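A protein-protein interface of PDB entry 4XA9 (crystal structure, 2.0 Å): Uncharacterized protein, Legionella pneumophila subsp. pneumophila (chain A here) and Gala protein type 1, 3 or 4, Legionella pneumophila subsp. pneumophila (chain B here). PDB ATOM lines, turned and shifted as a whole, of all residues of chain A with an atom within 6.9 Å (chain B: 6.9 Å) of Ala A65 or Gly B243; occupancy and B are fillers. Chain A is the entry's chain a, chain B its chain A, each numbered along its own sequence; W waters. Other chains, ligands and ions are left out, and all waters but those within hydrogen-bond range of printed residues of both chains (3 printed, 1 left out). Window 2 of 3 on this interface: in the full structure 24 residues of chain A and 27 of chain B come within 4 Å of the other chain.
Among the printed residues, merely in contact across the chains: Pro A66 with Ser B219 (3.5 Å), Gly A64 with Gly B243 (3.5 Å), Pro A66 with Gly B243 (3.5 Å), Ala A65 with Gly B243 (3.6 Å) and Ala A24 with Ile B242 (3.8 Å).
Of the 13 printed residues of chain B, 3 touch a printed residue of chain A.
Hydrophobic or aromatic side chains of chain B that line the printed part of chain A: Ile B242.
Hydrophobic or aromatic side chains of chain A within 4 Å of the printed part of chain B: Ala A24, Ala A65 and Pro A66.
Along chain A the printed residues that touch a printed residue of chain B span positions 24 to 66.
Among the printed residues, 5 pairs touch across the chains.
Gly A64 touches just one residue of chain B: Gly B243 (3.5 Å).
Of the printed residues of chain A, Ser B219 touches Pro A66.
Printed residues of chain A within 4 Å of Ile B242: Ala A24 (3.8 Å).
Gly B243 touches just these residues of chain A: Gly A64 (3.5 Å), Ala A65 (3.6 Å) and Pro A66 (3.5 Å).
The nearest printed residue of chain B that does not touch Ala A65 is Asn B244 (5.2 Å).
The nearest printed residue of chain B that does not touch Ala A24 is Asp B240 (5.0 Å).
Water W3 bridges the backbone carbonyl oxygen of Ala A24 (2.6 Å) and the side-chain carboxylate of Asp B240 (2.7 Å).
Water W2 bridges the side-chain hydroxyl of Ser B219 (2.6 Å) and the side-chain carboxylate of Glu A101 (2.9 Å).
Water W1 bridges O of Gly A64 (2.9 Å) and OG of Ser B219 (3.3 Å).
O of Ile B242 is in hydrogen-bond range of N of Ser B219 (2.9 Å).
N of Ile B242 is in hydrogen-bond range of OD1 of Asp B240, at 3.2 Å.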
ATOM      1  N   ALA A  24      -2.318  -2.413   7.134  1.00  0.00           N
ATOM      2  CA  ALA A  24      -1.098  -1.632   7.287  1.00  0.00           C
ATOM      3  C   ALA A  24      -0.963  -0.490   6.279  1.00  0.00           C
ATOM      4  O   ALA A  24      -0.309   0.510   6.579  1.00  0.00           O
ATOM      5  CB  ALA A  24       0.128  -2.550   7.213  1.00  0.00           C
ATOM      6  N   PHE A  60       5.199  -8.857  12.961  1.00  0.00           N
ATOM      7  CA  PHE A  60       4.263  -7.799  12.605  1.00  0.00           C
ATOM      8  C   PHE A  60       4.876  -6.828  11.604  1.00  0.00           C
ATOM      9  O   PHE A  60       4.237  -6.459  10.615  1.00  0.00           O
ATOM     10  CB  PHE A  60       3.795  -7.072  13.863  1.00  0.00           C
ATOM     11  CG  PHE A  60       3.241  -7.996  14.901  1.00  0.00           C
ATOM     12  CD1 PHE A  60       1.901  -8.346  14.890  1.00  0.00           C
ATOM     13  CD2 PHE A  60       4.068  -8.549  15.870  1.00  0.00           C
ATOM     14  CE1 PHE A  60       1.391  -9.217  15.835  1.00  0.00           C
ATOM     15  CE2 PHE A  60       3.563  -9.416  16.812  1.00  0.00           C
ATOM     16  CZ  PHE A  60       2.224  -9.754  16.791  1.00  0.00           C
ATOM     17  N   SER A  61       6.125  -6.446  11.850  1.00  0.00           N
ATOM     18  CA  SER A  61       6.837  -5.522  10.975  1.00  0.00           C
ATOM     19  C   SER A  61       6.897  -6.022   9.531  1.00  0.00           C
ATOM     20  O   SER A  61       6.705  -5.250   8.591  1.00  0.00           O
ATOM     21  CB  SER A  61       8.252  -5.281  11.501  1.00  0.00           C
ATOM     22  OG  SER A  61       8.951  -6.504  11.635  1.00  0.00           O
ATOM     23  N   GLN A  62       7.152  -7.313   9.350  1.00  0.00           N
ATOM     24  CA  GLN A  62       7.260  -7.865   8.005  1.00  0.00           C
ATOM     25  C   GLN A  62       5.878  -8.132   7.412  1.00  0.00           C
ATOM     26  O   GLN A  62       5.698  -8.064   6.198  1.00  0.00           O
ATOM     27  CB  GLN A  62       8.120  -9.135   8.013  1.00  0.00           C
ATOM     28  CG  GLN A  62       7.640 -10.225   8.955  1.00  0.00           C
ATOM     29  CD  GLN A  62       8.786 -10.931   9.662  1.00  0.00           C
ATOM     30  OE1 GLN A  62       9.901 -10.413   9.731  1.00  0.00           O
ATOM     31  NE2 GLN A  62       8.511 -12.112  10.205  1.00  0.00           N
ATOM     32  N   TRP A  63       4.899  -8.408   8.271  1.00  0.00           N
ATOM     33  CA  TRP A  63       3.516  -8.584   7.827  1.00  0.00           C
ATOM     34  C   TRP A  63       2.990  -7.336   7.117  1.00  0.00           C
ATOM     35  O   TRP A  63       2.136  -7.427   6.237  1.00  0.00           O
ATOM     36  CB  TRP A  63       2.605  -8.926   9.008  1.00  0.00           C
ATOM     37  CG  TRP A  63       2.654 -10.369   9.415  1.00  0.00           C
ATOM     38  CD1 TRP A  63       3.301 -11.382   8.769  1.00  0.00           C
ATOM     39  CD2 TRP A  63       2.039 -10.956  10.570  1.00  0.00           C
ATOM     40  NE1 TRP A  63       3.122 -12.564   9.446  1.00  0.00           N
ATOM     41  CE2 TRP A  63       2.351 -12.331  10.555  1.00  0.00           C
ATOM     42  CE3 TRP A  63       1.252 -10.452  11.613  1.00  0.00           C
ATOM     43  CZ2 TRP A  63       1.907 -13.210  11.544  1.00  0.00           C
ATOM     44  CZ3 TRP A  63       0.811 -11.327  12.594  1.00  0.00           C
ATOM     45  CH2 TRP A  63       1.138 -12.690  12.552  1.00  0.00           C
ATOM     46  N   GLY A  64       3.502  -6.172   7.506  1.00  0.00           N
ATOM     47  CA  GLY A  64       3.107  -4.927   6.875  1.00  0.00           C
ATOM     48  C   GLY A  64       3.833  -4.679   5.567  1.00  0.00           C
ATOM     49  O   GLY A  64       3.486  -3.768   4.822  1.00  0.00           O
ATOM     50  N   ALA A  65       4.845  -5.489   5.279  1.00  0.00           N
ATOM     51  CA  ALA A  65       5.646  -5.277   4.084  1.00  0.00           C
ATOM     52  C   ALA A  65       5.083  -6.048   2.895  1.00  0.00           C
ATOM     53  O   ALA A  65       4.690  -7.212   3.027  1.00  0.00           O
ATOM     54  CB  ALA A  65       7.090  -5.672   4.336  1.00  0.00           C
ATOM     55  N   PRO A  66       5.043  -5.394   1.725  1.00  0.00           N
ATOM     56  CA  PRO A  66       4.524  -6.007   0.500  1.00  0.00           C
ATOM     57  C   PRO A  66       5.276  -7.281   0.144  1.00  0.00           C
ATOM     58  O   PRO A  66       6.503  -7.304   0.202  1.00  0.00           O
ATOM     59  CB  PRO A  66       4.761  -4.928  -0.565  1.00  0.00           C
ATOM     60  CG  PRO A  66       4.868  -3.652   0.198  1.00  0.00           C
ATOM     61  CD  PRO A  66       5.516  -4.019   1.497  1.00  0.00           C
ATOM     62  N   GLN A  67       4.541  -8.330  -0.200  1.00  0.00           N
ATOM     63  CA  GLN A  67       5.144  -9.545  -0.724  1.00  0.00           C
ATOM     64  C   GLN A  67       4.900  -9.587  -2.228  1.00  0.00           C
ATOM     65  O   GLN A  67       3.857 -10.059  -2.681  1.00  0.00           O
ATOM     66  CB  GLN A  67       4.569 -10.783  -0.034  1.00  0.00           C
ATOM     67  CG  GLN A  67       5.485 -11.994  -0.065  1.00  0.00           C
ATOM     68  CD  GLN A  67       4.963 -13.142   0.776  1.00  0.00           C
ATOM     69  OE1 GLN A  67       3.854 -13.632   0.561  1.00  0.00           O
ATOM     70  NE2 GLN A  67       5.761 -13.574   1.745  1.00  0.00           N
ATOM     71  N   LEU A  68       5.862  -9.076  -2.995  1.00  0.00           N
ATOM     72  CA  LEU A  68       5.687  -8.898  -4.435  1.00  0.00           C
ATOM     73  C   LEU A  68       5.606 -10.220  -5.195  1.00  0.00           C
ATOM     74  O   LEU A  68       4.851 -10.337  -6.162  1.00  0.00           O
ATOM     75  CB  LEU A  68       6.821  -8.042  -5.006  1.00  0.00           C
ATOM     76  CG  LEU A  68       7.010  -6.658  -4.376  1.00  0.00           C
ATOM     77  CD1 LEU A  68       8.008  -5.832  -5.173  1.00  0.00           C
ATOM     78  CD2 LEU A  68       5.678  -5.930  -4.263  1.00  0.00           C
ATOM     79  N   ARG A  84      -1.094 -16.197   9.874  1.00  0.00           N
ATOM     80  CA  ARG A  84      -1.723 -14.916  10.167  1.00  0.00           C
ATOM     81  C   ARG A  84      -2.677 -15.018  11.348  1.00  0.00           C
ATOM     82  O   ARG A  84      -2.861 -14.055  12.086  1.00  0.00           O
ATOM     83  CB  ARG A  84      -2.481 -14.389   8.944  1.00  0.00           C
ATOM     84  CG  ARG A  84      -1.603 -13.750   7.894  1.00  0.00           C
ATOM     85  CD  ARG A  84      -0.722 -12.704   8.544  1.00  0.00           C
ATOM     86  NE  ARG A  84      -0.382 -11.597   7.653  1.00  0.00           N
ATOM     87  CZ  ARG A  84       0.601 -11.622   6.761  1.00  0.00           C
ATOM     88  NH1 ARG A  84       1.346 -12.710   6.615  1.00  0.00           N
ATOM     89  NH2 ARG A  84       0.834 -10.553   6.009  1.00  0.00           N
ATOM     90  N   VAL A  99      -2.139  -8.554  10.776  1.00  0.00           N
ATOM     91  CA  VAL A  99      -1.722  -7.465   9.897  1.00  0.00           C
ATOM     92  C   VAL A  99      -1.652  -7.910   8.447  1.00  0.00           C
ATOM     93  O   VAL A  99      -1.124  -8.980   8.159  1.00  0.00           O
ATOM     94  CB  VAL A  99      -0.340  -6.924  10.316  1.00  0.00           C
ATOM     95  CG1 VAL A  99       0.066  -5.749   9.446  1.00  0.00           C
ATOM     96  CG2 VAL A  99      -0.353  -6.520  11.789  1.00  0.00           C
ATOM     97  N   GLU A 101      -1.951  -6.178   3.999  1.00  0.00           N
ATOM     98  CA  GLU A 101      -1.998  -5.079   3.063  1.00  0.00           C
ATOM     99  C   GLU A 101      -2.557  -5.396   1.672  1.00  0.00           C
ATOM    100  O   GLU A 101      -3.026  -6.475   1.436  1.00  0.00           O
ATOM    101  CB  GLU A 101      -0.830  -4.122   3.139  1.00  0.00           C
ATOM    102  CG  GLU A 101       0.524  -4.713   2.985  1.00  0.00           C
ATOM    103  CD  GLU A 101       0.662  -5.388   1.682  1.00  0.00           C
ATOM    104  OE1 GLU A 101       0.321  -6.555   1.608  1.00  0.00           O
ATOM    105  OE2 GLU A 101       1.113  -4.730   0.752  1.00  0.00           O
ATOM    106  N   SER A 103      -1.458  -6.036  -1.173  1.00  0.00           N
ATOM    107  CA  SER A 103      -0.839  -7.019  -2.055  1.00  0.00           C
ATOM    108  C   SER A 103      -0.912  -8.446  -1.500  1.00  0.00           C
ATOM    109  O   SER A 103      -1.005  -9.399  -2.269  1.00  0.00           O
ATOM    110  CB  SER A 103       0.621  -6.652  -2.345  1.00  0.00           C
ATOM    111  OG  SER A 103       1.458  -6.913  -1.231  1.00  0.00           O
ATOM    112  N   ASN A 104      -0.875  -8.602  -0.178  1.00  0.00           N
ATOM    113  CA  ASN A 104      -0.843  -9.947   0.400  1.00  0.00           C
ATOM    114  C   ASN A 104      -2.170 -10.402   0.993  1.00  0.00           C
ATOM    115  O   ASN A 104      -2.328 -11.575   1.323  1.00  0.00           O
ATOM    116  CB  ASN A 104       0.259 -10.061   1.474  1.00  0.00           C
ATOM    117  CG  ASN A 104       0.033  -9.138   2.690  1.00  0.00           C
ATOM    118  OD1 ASN A 104      -1.060  -8.622   2.914  1.00  0.00           O
ATOM    119  ND2 ASN A 104       1.081  -8.948   3.484  1.00  0.00           N
ATOM    120  N   LEU B 217       5.773   7.481   4.189  1.00  0.00           N
ATOM    121  CA  LEU B 217       6.639   6.887   3.177  1.00  0.00           C
ATOM    122  C   LEU B 217       6.625   5.366   3.260  1.00  0.00           C
ATOM    123  O   LEU B 217       7.635   4.710   2.989  1.00  0.00           O
ATOM    124  CB  LEU B 217       8.075   7.404   3.330  1.00  0.00           C
ATOM    125  CG  LEU B 217       8.312   8.870   2.954  1.00  0.00           C
ATOM    126  CD1 LEU B 217       9.707   9.327   3.375  1.00  0.00           C
ATOM    127  CD2 LEU B 217       8.121   9.053   1.458  1.00  0.00           C
ATOM    128  N   GLY B 218       5.484   4.809   3.645  1.00  0.00           N
ATOM    129  CA  GLY B 218       5.360   3.369   3.790  1.00  0.00           C
ATOM    130  C   GLY B 218       5.619   2.591   2.510  1.00  0.00           C
ATOM    131  O   GLY B 218       5.451   3.117   1.408  1.00  0.00           O
ATOM    132  N   SER B 219       6.049   1.343   2.666  1.00  0.00           N
ATOM    133  CA  SER B 219       6.220   0.420   1.548  1.00  0.00           C
ATOM    134  C   SER B 219       7.040   1.005   0.408  1.00  0.00           C
ATOM    135  O   SER B 219       6.641   0.933  -0.755  1.00  0.00           O
ATOM    136  CB  SER B 219       4.857  -0.029   1.021  1.00  0.00           C
ATOM    137  OG  SER B 219       4.160  -0.754   2.014  1.00  0.00           O
ATOM    138  N   ASN B 220       8.170   1.610   0.751  1.00  0.00           N
ATOM    139  CA  ASN B 220       9.140   2.018  -0.243  1.00  0.00           C
ATOM    140  C   ASN B 220      10.392   1.165  -0.057  1.00  0.00           C
ATOM    141  O   ASN B 220      10.283   0.000   0.325  1.00  0.00           O
ATOM    142  CB  ASN B 220       9.444   3.514  -0.136  1.00  0.00           C
ATOM    143  CG  ASN B 220       8.355   4.379  -0.769  1.00  0.00           C
ATOM    144  OD1 ASN B 220       8.275   4.480  -1.988  1.00  0.00           O
ATOM    145  ND2 ASN B 220       7.541   5.025   0.056  1.00  0.00           N
ATOM    146  N   GLN B 221      11.569   1.734  -0.311  1.00  0.00           N
ATOM    147  CA  GLN B 221      12.819   0.983  -0.205  1.00  0.00           C
ATOM    148  C   GLN B 221      13.721   1.554   0.895  1.00  0.00           C
ATOM    149  O   GLN B 221      14.927   1.324   0.905  1.00  0.00           O
ATOM    150  CB  GLN B 221      13.567   0.998  -1.540  1.00  0.00           C
ATOM    151  CG  GLN B 221      12.773   0.464  -2.720  1.00  0.00           C
ATOM    152  CD  GLN B 221      13.501   0.666  -4.042  1.00  0.00           C
ATOM    153  OE1 GLN B 221      14.731   0.745  -4.088  1.00  0.00           O
ATOM    154  NE2 GLN B 221      12.737   0.770  -5.125  1.00  0.00           N
ATOM    155  N   ILE B 222      13.129   2.309   1.812  1.00  0.00           N
ATOM    156  CA  ILE B 222      13.894   2.995   2.844  1.00  0.00           C
ATOM    157  C   ILE B 222      14.444   1.982   3.853  1.00  0.00           C
ATOM    158  O   ILE B 222      13.751   1.034   4.221  1.00  0.00           O
ATOM    159  CB  ILE B 222      13.017   4.063   3.530  1.00  0.00           C
ATOM    160  CG1 ILE B 222      12.561   5.089   2.487  1.00  0.00           C
ATOM    161  CG2 ILE B 222      13.748   4.734   4.685  1.00  0.00           C
ATOM    162  CD1 ILE B 222      11.555   6.105   3.006  1.00  0.00           C
ATOM    163  N   ASP B 240       5.233   7.861   8.937  1.00  0.00           N
ATOM    164  CA  ASP B 240       4.876   6.464   8.676  1.00  0.00           C
ATOM    165  C   ASP B 240       5.872   5.782   7.748  1.00  0.00           C
ATOM    166  O   ASP B 240       6.086   6.214   6.612  1.00  0.00           O
ATOM    167  CB  ASP B 240       3.472   6.366   8.077  1.00  0.00           C
ATOM    168  CG  ASP B 240       3.076   4.932   7.749  1.00  0.00           C
ATOM    169  OD1 ASP B 240       3.501   4.013   8.479  1.00  0.00           O
ATOM    170  OD2 ASP B 240       2.346   4.725   6.754  1.00  0.00           O
ATOM    171  N   LEU B 241       6.468   4.700   8.238  1.00  0.00           N
ATOM    172  CA  LEU B 241       7.452   3.956   7.469  1.00  0.00           C
ATOM    173  C   LEU B 241       7.125   2.471   7.382  1.00  0.00           C
ATOM    174  O   LEU B 241       7.953   1.685   6.932  1.00  0.00           O
ATOM    175  CB  LEU B 241       8.836   4.139   8.083  1.00  0.00           C
ATOM    176  CG  LEU B 241       9.429   5.537   7.947  1.00  0.00           C
ATOM    177  CD1 LEU B 241      10.648   5.651   8.837  1.00  0.00           C
ATOM    178  CD2 LEU B 241       9.804   5.807   6.494  1.00  0.00           C
ATOM    179  N   ILE B 242       5.936   2.093   7.839  1.00  0.00           N
ATOM    180  CA  ILE B 242       5.492   0.700   7.794  1.00  0.00           C
ATOM    181  C   ILE B 242       5.734   0.070   6.425  1.00  0.00           C
ATOM    182  O   ILE B 242       5.406   0.664   5.400  1.00  0.00           O
ATOM    183  CB  ILE B 242       3.987   0.583   8.134  1.00  0.00           C
ATOM    184  CG1 ILE B 242       3.732   0.952   9.599  1.00  0.00           C
ATOM    185  CG2 ILE B 242       3.458  -0.820   7.809  1.00  0.00           C
ATOM    186  CD1 ILE B 242       2.266   0.936   9.982  1.00  0.00           C
ATOM    187  N   GLY B 243       6.316  -1.124   6.400  1.00  0.00           N
ATOM    188  CA  GLY B 243       6.436  -1.853   5.151  1.00  0.00           C
ATOM    189  C   GLY B 243       7.732  -1.636   4.395  1.00  0.00           C
ATOM    190  O   GLY B 243       7.966  -2.269   3.364  1.00  0.00           O
ATOM    191  N   ASN B 244       8.573  -0.736   4.897  1.00  0.00           N
ATOM    192  CA  ASN B 244       9.928  -0.568   4.369  1.00  0.00           C
ATOM    193  C   ASN B 244      10.872  -1.638   4.914  1.00  0.00           C
ATOM    194  O   ASN B 244      10.670  -2.135   6.025  1.00  0.00           O
ATOM    195  CB  ASN B 244      10.486   0.820   4.709  1.00  0.00           C
ATOM    196  CG  ASN B 244       9.821   1.923   3.924  1.00  0.00           C
ATOM    197  OD1 ASN B 244      10.150   2.151   2.761  1.00  0.00           O
ATOM    198  ND2 ASN B 244       8.887   2.625   4.560  1.00  0.00           N
ATOM    199  N   PRO B 245      11.913  -1.991   4.138  1.00  0.00           N
ATOM    200  CA  PRO B 245      12.895  -2.984   4.600  1.00  0.00           C
ATOM    201  C   PRO B 245      13.824  -2.412   5.671  1.00  0.00           C
ATOM    202  O   PRO B 245      15.010  -2.192   5.423  1.00  0.00           O
ATOM    203  CB  PRO B 245      13.671  -3.326   3.326  1.00  0.00           C
ATOM    204  CG  PRO B 245      13.580  -2.088   2.492  1.00  0.00           C
ATOM    205  CD  PRO B 245      12.211  -1.510   2.776  1.00  0.00           C
ATOM    206  N   ILE B 246      13.275  -2.174   6.854  1.00  0.00           N
ATOM    207  CA  ILE B 246      14.028  -1.591   7.958  1.00  0.00           C
ATOM    208  C   ILE B 246      14.597  -2.677   8.877  1.00  0.00           C
ATOM    209  O   ILE B 246      13.886  -3.603   9.255  1.00  0.00           O
ATOM    210  CB  ILE B 246      13.139  -0.627   8.773  1.00  0.00           C
ATOM    211  CG1 ILE B 246      12.617   0.498   7.869  1.00  0.00           C
ATOM    212  CG2 ILE B 246      13.888  -0.085   9.985  1.00  0.00           C
ATOM    213  CD1 ILE B 246      11.693   1.488   8.562  1.00  0.00           C
HETATM  214  O   HOH W   1       1.789  -1.584   4.109  1.00  0.00           O
HETATM  215  O   HOH W   2       1.971  -2.123   1.551  1.00  0.00           O
HETATM  216  O   HOH W   3       1.269   2.450   5.925  1.00  0.00           O
